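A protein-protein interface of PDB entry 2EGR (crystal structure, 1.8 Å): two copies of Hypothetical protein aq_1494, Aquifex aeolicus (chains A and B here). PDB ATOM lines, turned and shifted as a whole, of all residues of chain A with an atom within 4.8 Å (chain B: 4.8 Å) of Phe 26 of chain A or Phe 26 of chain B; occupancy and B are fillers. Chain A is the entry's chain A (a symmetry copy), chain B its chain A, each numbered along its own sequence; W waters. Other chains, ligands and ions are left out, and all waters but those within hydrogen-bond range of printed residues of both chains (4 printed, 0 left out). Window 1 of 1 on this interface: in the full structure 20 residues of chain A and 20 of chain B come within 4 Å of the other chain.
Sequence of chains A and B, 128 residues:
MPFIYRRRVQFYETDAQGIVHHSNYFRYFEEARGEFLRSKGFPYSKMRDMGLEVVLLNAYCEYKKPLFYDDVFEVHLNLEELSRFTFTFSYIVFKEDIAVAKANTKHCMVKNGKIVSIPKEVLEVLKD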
ATOM      1  N   HIS A  22     -15.502 -13.425   1.628  1.00  0.00           N
ATOM      2  CA  HIS A  22     -15.906 -14.814   1.899  1.00  0.00           C
ATOM      3  C   HIS A  22     -15.306 -15.438   3.174  1.00  0.00           C
ATOM      4  O   HIS A  22     -15.932 -16.274   3.825  1.00  0.00           O
ATOM      5  CB  HIS A  22     -15.666 -15.735   0.684  1.00  0.00           C
ATOM      6  CG  HIS A  22     -14.218 -15.908   0.309  1.00  0.00           C
ATOM      7  ND1 HIS A  22     -13.555 -15.024  -0.514  1.00  0.00           N
ATOM      8  CD2 HIS A  22     -13.323 -16.869   0.625  1.00  0.00           C
ATOM      9  CE1 HIS A  22     -12.310 -15.437  -0.686  1.00  0.00           C
ATOM     10  NE2 HIS A  22     -12.145 -16.559  -0.008  1.00  0.00           N
ATOM     11  N   SER A  23     -14.077 -15.025   3.549  1.00  0.00           N
ATOM     12  CA  SER A  23     -13.418 -15.596   4.673  1.00  0.00           C
ATOM     13  C   SER A  23     -14.106 -15.188   5.987  1.00  0.00           C
ATOM     14  O   SER A  23     -13.933 -15.851   6.969  1.00  0.00           O
ATOM     15  CB  SER A  23     -11.944 -15.156   4.721  1.00  0.00           C
ATOM     16  OG  SER A  23     -11.847 -13.761   4.993  1.00  0.00           O
ATOM     17  N   ASN A  24     -14.829 -14.071   5.984  1.00  0.00           N
ATOM     18  CA  ASN A  24     -15.447 -13.562   7.221  1.00  0.00           C
ATOM     19  C   ASN A  24     -16.670 -14.391   7.600  1.00  0.00           C
ATOM     20  O   ASN A  24     -17.082 -14.378   8.754  1.00  0.00           O
ATOM     21  CB  ASN A  24     -15.851 -12.080   7.076  1.00  0.00           C
ATOM     22  CG  ASN A  24     -14.629 -11.138   7.069  1.00  0.00           C
ATOM     23  OD1 ASN A  24     -14.623 -10.075   6.431  1.00  0.00           O
ATOM     24  ND2 ASN A  24     -13.631 -11.520   7.788  1.00  0.00           N
ATOM     25  N   TYR A  25     -17.260 -15.089   6.635  1.00  0.00           N
ATOM     26  CA  TYR A  25     -18.396 -15.989   6.971  1.00  0.00           C
ATOM     27  C   TYR A  25     -17.991 -17.017   7.992  1.00  0.00           C
ATOM     28  O   TYR A  25     -18.752 -17.289   8.920  1.00  0.00           O
ATOM     29  CB  TYR A  25     -19.021 -16.632   5.710  1.00  0.00           C
ATOM     30  CG  TYR A  25     -19.804 -15.688   4.848  1.00  0.00           C
ATOM     31  CD1 TYR A  25     -21.213 -15.800   4.776  1.00  0.00           C
ATOM     32  CD2 TYR A  25     -19.171 -14.686   4.081  1.00  0.00           C
ATOM     33  CE1 TYR A  25     -21.953 -14.948   3.974  1.00  0.00           C
ATOM     34  CE2 TYR A  25     -19.914 -13.788   3.249  1.00  0.00           C
ATOM     35  CZ  TYR A  25     -21.315 -13.959   3.199  1.00  0.00           C
ATOM     36  OH  TYR A  25     -22.077 -13.142   2.410  1.00  0.00           O
ATOM     37  N   PHE A  26     -16.752 -17.549   7.900  1.00  0.00           N
ATOM     38  CA  PHE A  26     -16.267 -18.494   8.893  1.00  0.00           C
ATOM     39  C   PHE A  26     -16.170 -17.868  10.274  1.00  0.00           C
ATOM     40  O   PHE A  26     -16.403 -18.540  11.268  1.00  0.00           O
ATOM     41  CB  PHE A  26     -14.963 -19.147   8.441  1.00  0.00           C
ATOM     42  CG  PHE A  26     -15.133 -19.874   7.145  1.00  0.00           C
ATOM     43  CD1 PHE A  26     -15.747 -21.153   7.121  1.00  0.00           C
ATOM     44  CD2 PHE A  26     -14.815 -19.244   5.939  1.00  0.00           C
ATOM     45  CE1 PHE A  26     -15.951 -21.799   5.893  1.00  0.00           C
ATOM     46  CE2 PHE A  26     -15.053 -19.877   4.700  1.00  0.00           C
ATOM     47  CZ  PHE A  26     -15.613 -21.166   4.691  1.00  0.00           C
ATOM     48  N   ARG A  27     -15.843 -16.577  10.314  1.00  0.00           N
ATOM     49  CA  ARG A  27     -15.794 -15.846  11.592  1.00  0.00           C
ATOM     50  C   ARG A  27     -17.185 -15.694  12.200  1.00  0.00           C
ATOM     51  O   ARG A  27     -17.356 -15.917  13.420  1.00  0.00           O
ATOM     52  CB  ARG A  27     -15.101 -14.504  11.391  1.00  0.00           C
ATOM     53  CG  ARG A  27     -13.642 -14.714  10.907  1.00  0.00           C
ATOM     54  CD  ARG A  27     -12.906 -13.377  10.600  1.00  0.00           C
ATOM     55  NE  ARG A  27     -11.495 -13.688  10.236  1.00  0.00           N
ATOM     56  CZ  ARG A  27     -10.478 -12.831  10.352  1.00  0.00           C
ATOM     57  NH1 ARG A  27     -10.724 -11.564  10.736  1.00  0.00           N
ATOM     58  NH2 ARG A  27      -9.220 -13.235  10.029  1.00  0.00           N
ATOM     59  N   TYR A  28     -18.158 -15.369  11.348  1.00  0.00           N
ATOM     60  CA  TYR A  28     -19.557 -15.305  11.755  1.00  0.00           C
ATOM     61  C   TYR A  28     -20.017 -16.648  12.305  1.00  0.00           C
ATOM     62  O   TYR A  28     -20.660 -16.677  13.349  1.00  0.00           O
ATOM     63  CB  TYR A  28     -20.465 -14.917  10.601  1.00  0.00           C
ATOM     64  CG  TYR A  28     -20.289 -13.545   9.980  1.00  0.00           C
ATOM     65  CD1 TYR A  28     -19.707 -12.491  10.677  1.00  0.00           C
ATOM     66  CD2 TYR A  28     -20.746 -13.321   8.690  1.00  0.00           C
ATOM     67  CE1 TYR A  28     -19.607 -11.213  10.081  1.00  0.00           C
ATOM     68  CE2 TYR A  28     -20.670 -12.094   8.083  1.00  0.00           C
ATOM     69  CZ  TYR A  28     -20.087 -11.032   8.798  1.00  0.00           C
ATOM     70  OH  TYR A  28     -20.030  -9.798   8.189  1.00  0.00           O
ATOM     71  N   PHE A  29     -19.664 -17.760  11.639  1.00  0.00           N
ATOM     72  CA  PHE A  29     -20.020 -19.103  12.182  1.00  0.00           C
ATOM     73  C   PHE A  29     -19.404 -19.359  13.540  1.00  0.00           C
ATOM     74  O   PHE A  29     -20.018 -19.980  14.411  1.00  0.00           O
ATOM     75  CB  PHE A  29     -19.632 -20.225  11.195  1.00  0.00           C
ATOM     76  CG  PHE A  29     -20.138 -20.008   9.818  1.00  0.00           C
ATOM     77  CD1 PHE A  29     -21.363 -19.358   9.582  1.00  0.00           C
ATOM     78  CD2 PHE A  29     -19.402 -20.452   8.711  1.00  0.00           C
ATOM     79  CE1 PHE A  29     -21.825 -19.137   8.303  1.00  0.00           C
ATOM     80  CE2 PHE A  29     -19.871 -20.237   7.430  1.00  0.00           C
ATOM     81  CZ  PHE A  29     -21.075 -19.586   7.204  1.00  0.00           C
ATOM     82  N   GLU A  30     -18.155 -18.918  13.750  1.00  0.00           N
ATOM     83  CA  GLU A  30     -17.521 -19.075  15.025  1.00  0.00           C
ATOM     84  C   GLU A  30     -18.278 -18.249  16.066  1.00  0.00           C
ATOM     85  O   GLU A  30     -18.524 -18.732  17.183  1.00  0.00           O
ATOM     86  CB  GLU A  30     -16.045 -18.622  14.949  1.00  0.00           C
ATOM     87  CG  GLU A  30     -15.303 -18.647  16.284  1.00  0.00           C
ATOM     88  CD  GLU A  30     -13.932 -17.990  16.198  1.00  0.00           C
ATOM     89  OE1 GLU A  30     -12.983 -18.641  15.678  1.00  0.00           O
ATOM     90  OE2 GLU A  30     -13.837 -16.852  16.688  1.00  0.00           O
ATOM     91  N   ALA A  59     -14.247 -27.397   6.952  1.00  0.00           N
ATOM     92  CA  ALA A  59     -15.282 -26.372   6.821  1.00  0.00           C
ATOM     93  C   ALA A  59     -15.621 -26.162   5.357  1.00  0.00           C
ATOM     94  O   ALA A  59     -14.727 -26.228   4.477  1.00  0.00           O
ATOM     95  CB  ALA A  59     -14.802 -25.039   7.478  1.00  0.00           C
ATOM     96  N   TYR A  60     -16.886 -25.858   5.097  1.00  0.00           N
ATOM     97  CA  TYR A  60     -17.410 -25.694   3.778  1.00  0.00           C
ATOM     98  C   TYR A  60     -18.403 -24.541   3.796  1.00  0.00           C
ATOM     99  O   TYR A  60     -19.218 -24.414   4.733  1.00  0.00           O
ATOM    100  CB  TYR A  60     -18.149 -26.978   3.332  1.00  0.00           C
ATOM    101  CG  TYR A  60     -18.912 -26.798   2.047  1.00  0.00           C
ATOM    102  CD1 TYR A  60     -18.243 -26.803   0.807  1.00  0.00           C
ATOM    103  CD2 TYR A  60     -20.284 -26.567   2.049  1.00  0.00           C
ATOM    104  CE1 TYR A  60     -18.947 -26.621  -0.388  1.00  0.00           C
ATOM    105  CE2 TYR A  60     -20.991 -26.394   0.863  1.00  0.00           C
ATOM    106  CZ  TYR A  60     -20.316 -26.436  -0.350  1.00  0.00           C
ATOM    107  OH  TYR A  60     -21.001 -26.222  -1.524  1.00  0.00           O
ATOM    108  N   CYS A  61     -18.340 -23.689   2.780  1.00  0.00           N
ATOM    109  CA  CYS A  61     -19.351 -22.652   2.604  1.00  0.00           C
ATOM    110  C   CYS A  61     -19.728 -22.496   1.146  1.00  0.00           C
ATOM    111  O   CYS A  61     -18.849 -22.491   0.264  1.00  0.00           O
ATOM    112  CB  CYS A  61     -18.928 -21.291   3.208  1.00  0.00           C
ATOM    113  SG  CYS A  61     -20.311 -20.126   3.397  1.00  0.00           S
ATOM    114  N   TYR A  63     -21.929 -19.917  -1.334  1.00  0.00           N
ATOM    115  CA  TYR A  63     -22.291 -18.516  -1.373  1.00  0.00           C
ATOM    116  C   TYR A  63     -23.320 -18.270  -2.461  1.00  0.00           C
ATOM    117  O   TYR A  63     -23.046 -18.423  -3.660  1.00  0.00           O
ATOM    118  CB  TYR A  63     -21.043 -17.629  -1.578  1.00  0.00           C
ATOM    119  CG  TYR A  63     -19.950 -17.829  -0.535  1.00  0.00           C
ATOM    120  CD1 TYR A  63     -19.863 -16.987   0.578  1.00  0.00           C
ATOM    121  CD2 TYR A  63     -19.012 -18.857  -0.668  1.00  0.00           C
ATOM    122  CE1 TYR A  63     -18.855 -17.178   1.551  1.00  0.00           C
ATOM    123  CE2 TYR A  63     -18.026 -19.082   0.294  1.00  0.00           C
ATOM    124  CZ  TYR A  63     -17.948 -18.218   1.409  1.00  0.00           C
ATOM    125  OH  TYR A  63     -16.970 -18.423   2.340  1.00  0.00           O
ATOM    126  N   HIS B  22      -8.444 -20.599  11.232  1.00  0.00           N
ATOM    127  CA  HIS B  22      -8.914 -21.312  10.034  1.00  0.00           C
ATOM    128  C   HIS B  22      -9.400 -20.412   8.879  1.00  0.00           C
ATOM    129  O   HIS B  22      -9.266 -20.760   7.707  1.00  0.00           O
ATOM    130  CB  HIS B  22      -9.979 -22.376  10.372  1.00  0.00           C
ATOM    131  CG  HIS B  22     -11.267 -21.817  10.918  1.00  0.00           C
ATOM    132  ND1 HIS B  22     -11.446 -21.537  12.255  1.00  0.00           N
ATOM    133  CD2 HIS B  22     -12.435 -21.513  10.312  1.00  0.00           C
ATOM    134  CE1 HIS B  22     -12.673 -21.081  12.446  1.00  0.00           C
ATOM    135  NE2 HIS B  22     -13.296 -21.062  11.280  1.00  0.00           N
ATOM    136  N   SER B  23      -9.965 -19.232   9.208  1.00  0.00           N
ATOM    137  CA  SER B  23     -10.503 -18.370   8.212  1.00  0.00           C
ATOM    138  C   SER B  23      -9.388 -17.752   7.351  1.00  0.00           C
ATOM    139  O   SER B  23      -9.658 -17.320   6.267  1.00  0.00           O
ATOM    140  CB  SER B  23     -11.324 -17.239   8.858  1.00  0.00           C
ATOM    141  OG  SER B  23     -10.475 -16.359   9.589  1.00  0.00           O
ATOM    142  N   ASN B  24      -8.169 -17.678   7.880  1.00  0.00           N
ATOM    143  CA  ASN B  24      -7.067 -17.020   7.158  1.00  0.00           C
ATOM    144  C   ASN B  24      -6.556 -17.903   6.024  1.00  0.00           C
ATOM    145  O   ASN B  24      -5.930 -17.402   5.096  1.00  0.00           O
ATOM    146  CB  ASN B  24      -5.903 -16.674   8.110  1.00  0.00           C
ATOM    147  CG  ASN B  24      -6.244 -15.500   9.050  1.00  0.00           C
ATOM    148  OD1 ASN B  24      -5.773 -15.416  10.195  1.00  0.00           O
ATOM    149  ND2 ASN B  24      -7.029 -14.606   8.557  1.00  0.00           N
ATOM    150  N   TYR B  25      -6.799 -19.207   6.105  1.00  0.00           N
ATOM    151  CA  TYR B  25      -6.407 -20.097   4.979  1.00  0.00           C
ATOM    152  C   TYR B  25      -7.061 -19.666   3.694  1.00  0.00           C
ATOM    153  O   TYR B  25      -6.408 -19.656   2.650  1.00  0.00           O
ATOM    154  CB  TYR B  25      -6.670 -21.588   5.299  1.00  0.00           C
ATOM    155  CG  TYR B  25      -5.743 -22.184   6.313  1.00  0.00           C
ATOM    156  CD1 TYR B  25      -4.777 -23.139   5.915  1.00  0.00           C
ATOM    157  CD2 TYR B  25      -5.812 -21.830   7.679  1.00  0.00           C
ATOM    158  CE1 TYR B  25      -3.921 -23.713   6.840  1.00  0.00           C
ATOM    159  CE2 TYR B  25      -4.934 -22.405   8.654  1.00  0.00           C
ATOM    160  CZ  TYR B  25      -4.005 -23.368   8.204  1.00  0.00           C
ATOM    161  OH  TYR B  25      -3.149 -23.963   9.090  1.00  0.00           O
ATOM    162  N   PHE B  26      -8.335 -19.218   3.749  1.00  0.00           N
ATOM    163  CA  PHE B  26      -9.006 -18.720   2.559  1.00  0.00           C
ATOM    164  C   PHE B  26      -8.326 -17.480   2.002  1.00  0.00           C
ATOM    165  O   PHE B  26      -8.294 -17.291   0.794  1.00  0.00           O
ATOM    166  CB  PHE B  26     -10.498 -18.520   2.811  1.00  0.00           C
ATOM    167  CG  PHE B  26     -11.160 -19.796   3.223  1.00  0.00           C
ATOM    168  CD1 PHE B  26     -11.487 -20.776   2.251  1.00  0.00           C
ATOM    169  CD2 PHE B  26     -11.339 -20.090   4.578  1.00  0.00           C
ATOM    170  CE1 PHE B  26     -12.056 -21.990   2.657  1.00  0.00           C
ATOM    171  CE2 PHE B  26     -11.878 -21.326   4.991  1.00  0.00           C
ATOM    172  CZ  PHE B  26     -12.247 -22.268   4.016  1.00  0.00           C
ATOM    173  N   ARG B  27      -7.775 -16.659   2.894  1.00  0.00           N
ATOM    174  CA  ARG B  27      -7.024 -15.466   2.465  1.00  0.00           C
ATOM    175  C   ARG B  27      -5.728 -15.849   1.754  1.00  0.00           C
ATOM    176  O   ARG B  27      -5.409 -15.270   0.692  1.00  0.00           O
ATOM    177  CB  ARG B  27      -6.779 -14.554   3.660  1.00  0.00           C
ATOM    178  CG  ARG B  27      -8.126 -14.076   4.263  1.00  0.00           C
ATOM    179  CD  ARG B  27      -7.945 -13.208   5.542  1.00  0.00           C
ATOM    180  NE  ARG B  27      -9.286 -12.729   5.981  1.00  0.00           N
ATOM    181  CZ  ARG B  27      -9.493 -11.639   6.724  1.00  0.00           C
ATOM    182  NH1 ARG B  27      -8.436 -10.955   7.201  1.00  0.00           N
ATOM    183  NH2 ARG B  27     -10.766 -11.269   7.032  1.00  0.00           N
ATOM    184  N   TYR B  28      -5.033 -16.841   2.312  1.00  0.00           N
ATOM    185  CA  TYR B  28      -3.839 -17.400   1.688  1.00  0.00           C
ATOM    186  C   TYR B  28      -4.165 -17.946   0.304  1.00  0.00           C
ATOM    187  O   TYR B  28      -3.422 -17.676  -0.635  1.00  0.00           O
ATOM    188  CB  TYR B  28      -3.236 -18.517   2.519  1.00  0.00           C
ATOM    189  CG  TYR B  28      -2.699 -18.176   3.896  1.00  0.00           C
ATOM    190  CD1 TYR B  28      -2.305 -16.885   4.234  1.00  0.00           C
ATOM    191  CD2 TYR B  28      -2.567 -19.184   4.841  1.00  0.00           C
ATOM    192  CE1 TYR B  28      -1.763 -16.619   5.511  1.00  0.00           C
ATOM    193  CE2 TYR B  28      -2.041 -18.962   6.087  1.00  0.00           C
ATOM    194  CZ  TYR B  28      -1.638 -17.655   6.417  1.00  0.00           C
ATOM    195  OH  TYR B  28      -1.094 -17.443   7.665  1.00  0.00           O
ATOM    196  N   PHE B  29      -5.284 -18.674   0.157  1.00  0.00           N
ATOM    197  CA  PHE B  29      -5.689 -19.161  -1.193  1.00  0.00           C
ATOM    198  C   PHE B  29      -5.940 -18.029  -2.165  1.00  0.00           C
ATOM    199  O   PHE B  29      -5.626 -18.127  -3.352  1.00  0.00           O
ATOM    200  CB  PHE B  29      -6.927 -20.080  -1.108  1.00  0.00           C
ATOM    201  CG  PHE B  29      -6.786 -21.177  -0.118  1.00  0.00           C
ATOM    202  CD1 PHE B  29      -5.539 -21.774   0.141  1.00  0.00           C
ATOM    203  CD2 PHE B  29      -7.903 -21.649   0.584  1.00  0.00           C
ATOM    204  CE1 PHE B  29      -5.403 -22.778   1.074  1.00  0.00           C
ATOM    205  CE2 PHE B  29      -7.766 -22.661   1.514  1.00  0.00           C
ATOM    206  CZ  PHE B  29      -6.531 -23.238   1.772  1.00  0.00           C
ATOM    207  N   GLU B  30      -6.549 -16.929  -1.695  1.00  0.00           N
ATOM    208  CA  GLU B  30      -6.776 -15.794  -2.539  1.00  0.00           C
ATOM    209  C   GLU B  30      -5.428 -15.201  -2.952  1.00  0.00           C
ATOM    210  O   GLU B  30      -5.239 -14.853  -4.130  1.00  0.00           O
ATOM    211  CB  GLU B  30      -7.624 -14.735  -1.795  1.00  0.00           C
ATOM    212  CG  GLU B  30      -7.835 -13.435  -2.567  1.00  0.00           C
ATOM    213  CD  GLU B  30      -8.482 -12.353  -1.713  1.00  0.00           C
ATOM    214  OE1 GLU B  30      -9.727 -12.411  -1.507  1.00  0.00           O
ATOM    215  OE2 GLU B  30      -7.729 -11.452  -1.304  1.00  0.00           O
ATOM    216  N   ALA B  59     -16.449 -22.858  -1.255  1.00  0.00           N
ATOM    217  CA  ALA B  59     -15.088 -23.099  -0.778  1.00  0.00           C
ATOM    218  C   ALA B  59     -15.101 -24.153   0.314  1.00  0.00           C
ATOM    219  O   ALA B  59     -16.045 -24.207   1.140  1.00  0.00           O
ATOM    220  CB  ALA B  59     -14.461 -21.767  -0.259  1.00  0.00           C
ATOM    221  N   TYR B  60     -14.041 -24.949   0.356  1.00  0.00           N
ATOM    222  CA  TYR B  60     -13.904 -26.043   1.265  1.00  0.00           C
ATOM    223  C   TYR B  60     -12.455 -26.103   1.730  1.00  0.00           C
ATOM    224  O   TYR B  60     -11.518 -25.935   0.922  1.00  0.00           O
ATOM    225  CB  TYR B  60     -14.252 -27.374   0.557  1.00  0.00           C
ATOM    226  CG  TYR B  60     -13.917 -28.584   1.388  1.00  0.00           C
ATOM    227  CD1 TYR B  60     -14.753 -28.980   2.450  1.00  0.00           C
ATOM    228  CD2 TYR B  60     -12.751 -29.311   1.166  1.00  0.00           C
ATOM    229  CE1 TYR B  60     -14.437 -30.095   3.234  1.00  0.00           C
ATOM    230  CE2 TYR B  60     -12.437 -30.426   1.936  1.00  0.00           C
ATOM    231  CZ  TYR B  60     -13.292 -30.817   2.958  1.00  0.00           C
ATOM    232  OH  TYR B  60     -12.965 -31.893   3.752  1.00  0.00           O
ATOM    233  N   CYS B  61     -12.258 -26.326   3.022  1.00  0.00           N
ATOM    234  CA  CYS B  61     -10.918 -26.575   3.546  1.00  0.00           C
ATOM    235  C   CYS B  61     -10.934 -27.673   4.589  1.00  0.00           C
ATOM    236  O   CYS B  61     -11.824 -27.705   5.458  1.00  0.00           O
ATOM    237  CB  CYS B  61     -10.245 -25.299   4.107  1.00  0.00           C
ATOM    238  SG  CYS B  61      -8.452 -25.480   4.352  1.00  0.00           S
ATOM    239  N   TYR B  63      -8.386 -29.421   7.435  1.00  0.00           N
ATOM    240  CA  TYR B  63      -7.274 -29.019   8.271  1.00  0.00           C
ATOM    241  C   TYR B  63      -6.648 -30.232   8.931  1.00  0.00           C
ATOM    242  O   TYR B  63      -7.267 -30.911   9.764  1.00  0.00           O
ATOM    243  CB  TYR B  63      -7.722 -27.981   9.325  1.00  0.00           C
ATOM    244  CG  TYR B  63      -8.381 -26.736   8.743  1.00  0.00           C
ATOM    245  CD1 TYR B  63      -7.634 -25.576   8.514  1.00  0.00           C
ATOM    246  CD2 TYR B  63      -9.741 -26.726   8.426  1.00  0.00           C
ATOM    247  CE1 TYR B  63      -8.242 -24.423   7.965  1.00  0.00           C
ATOM    248  CE2 TYR B  63     -10.357 -25.610   7.857  1.00  0.00           C
ATOM    249  CZ  TYR B  63      -9.590 -24.444   7.638  1.00  0.00           C
ATOM    250  OH  TYR B  63     -10.196 -23.343   7.103  1.00  0.00           O
HETATM  251  O   HOH W   1     -10.024 -18.055  -1.055  1.00  0.00           O
HETATM  252  O   HOH W   2      -7.029 -11.488  10.330  1.00  0.00           O
HETATM  253  O   HOH W   3     -11.258  -8.935   8.532  1.00  0.00           O
HETATM  254  O   HOH W   4     -16.072 -21.139  11.633  1.00  0.00           O
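The guanidinium group of Arg 27 of chain A is in hydrogen-bond range of the side-chain hydroxyl of Ser 23 of chain B, 2.9 Å away.
The side-chain amide nitrogen (ND2) of Asn 24 of chain B sits close to the guanidinium group (NH2) of Arg 27 of chain A (3.0 Å).
OG of Ser 23 of chain A is in hydrogen-bond range of NE of Arg 27 of chain B (2.9 Å).
NH2 of Arg 27 of chain B lies close to ND2 of Asn 24 of chain A, 3.0 Å away.
N of Ala 59 of chain B sits at hydrogen-bond distance from O of Cys 61 of chain A (2.9 Å).
The backbone carbonyl oxygen (O) of Cys 61 of chain B is in hydrogen-bond range of the backbone NH (N) of Ala 59 of chain A, at 2.9 Å.
Of the printed residues of chain B, Phe 26 of chain A touches His 22 (3.8 Å) and Phe 26 (3.5 Å).
Of the printed residues of chain B, Cys 61 of chain A touches Ala 59 (2.9 Å).
Printed residues of chain A within 4 Å of Ser 23 of chain B: Ser 23 (3.5 Å) and Arg 27 (2.9 Å).
Of chain A, only His 22 and Phe 26 come within 4 Å of Phe 26 of chain B.
The nearest residue of chain B that does not touch Phe 26 of chain A is Ser 23 of chain B (4.1 Å).
The nearest printed residue of chain A that does not touch Ser 23 of chain B is Phe 26 of chain A (4.1 Å).
Among the printed residues, pairs that only touch across the chains: Ala 59 of chain A with Tyr 60 of chain B (3.3 Å), Tyr 60 of chain A with Ala 59 of chain B (3.3 Å), Phe 26 of chain A with Phe 26 of chain B (3.5 Å), Ser 23 of chain A with Ser 23 of chain B (3.5 Å), Arg 27 of chain A with Arg 27 of chain B (3.7 Å), His 22 of chain A with Phe 26 of chain B (3.8 Å) and Phe 26 of chain A with His 22 of chain B (3.8 Å).
The backbone carbonyl oxygen (O) of His 22 of chain B sits at hydrogen-bond distance from the side-chain hydroxyl (OH) of Tyr 63 of chain B (2.8 Å).
OH of Tyr 63 of chain A is in hydrogen-bond range of O of His 22 of chain A (2.8 Å).
Asn 24 of chain A touches Arg 27 of chain B, and with the chains exchanged Arg 27 of chain A touches Asn 24 of chain B.
Phe 26 of chain B touches its own counterpart, Phe 26 of chain A.
Ala 59 of chain A touches Tyr 60 of chain B, and with the chains exchanged Tyr 60 of chain A touches Ala 59 of chain B.
Ala 59 of chain A touches Cys 61 of chain B, and with the chains exchanged Cys 61 of chain A touches Ala 59 of chain B.
13 positions are printed for both chains.
Of the 13 pairs that touch across the chains among the printed residues, 13 have their exchanged pair printed and touching as well.
Hydrophobic or aromatic side chains of chain A that line the printed part of chain B: His 22, Phe 26 and Tyr 60.
Among the printed residues, no Asp or Glu carboxylate lies within 4 Å of a Lys or Arg side-chain nitrogen of the other chain.
Water W4 bridges the backbone carbonyl oxygen (O) of Phe 26 of chain A (2.6 Å) and a ring nitrogen (NE2) of His 22 of chain B (2.8 Å).
Water W1 bridges O of Phe 26 of chain B (2.6 Å) and NE2 of His 22 of chain A (2.8 Å).
Water W3 lies within hydrogen-bond range of the guanidinium group (NH2) of Arg 27 of chain B (2.8 Å) and the guanidinium group (NH1) of Arg 27 of chain A (3.5 Å).
Water W2 lies within hydrogen-bond range of the guanidinium group (NH2) of Arg 27 of chain A (2.8 Å) and the guanidinium group (NH1) of Arg 27 of chain B (3.5 Å).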
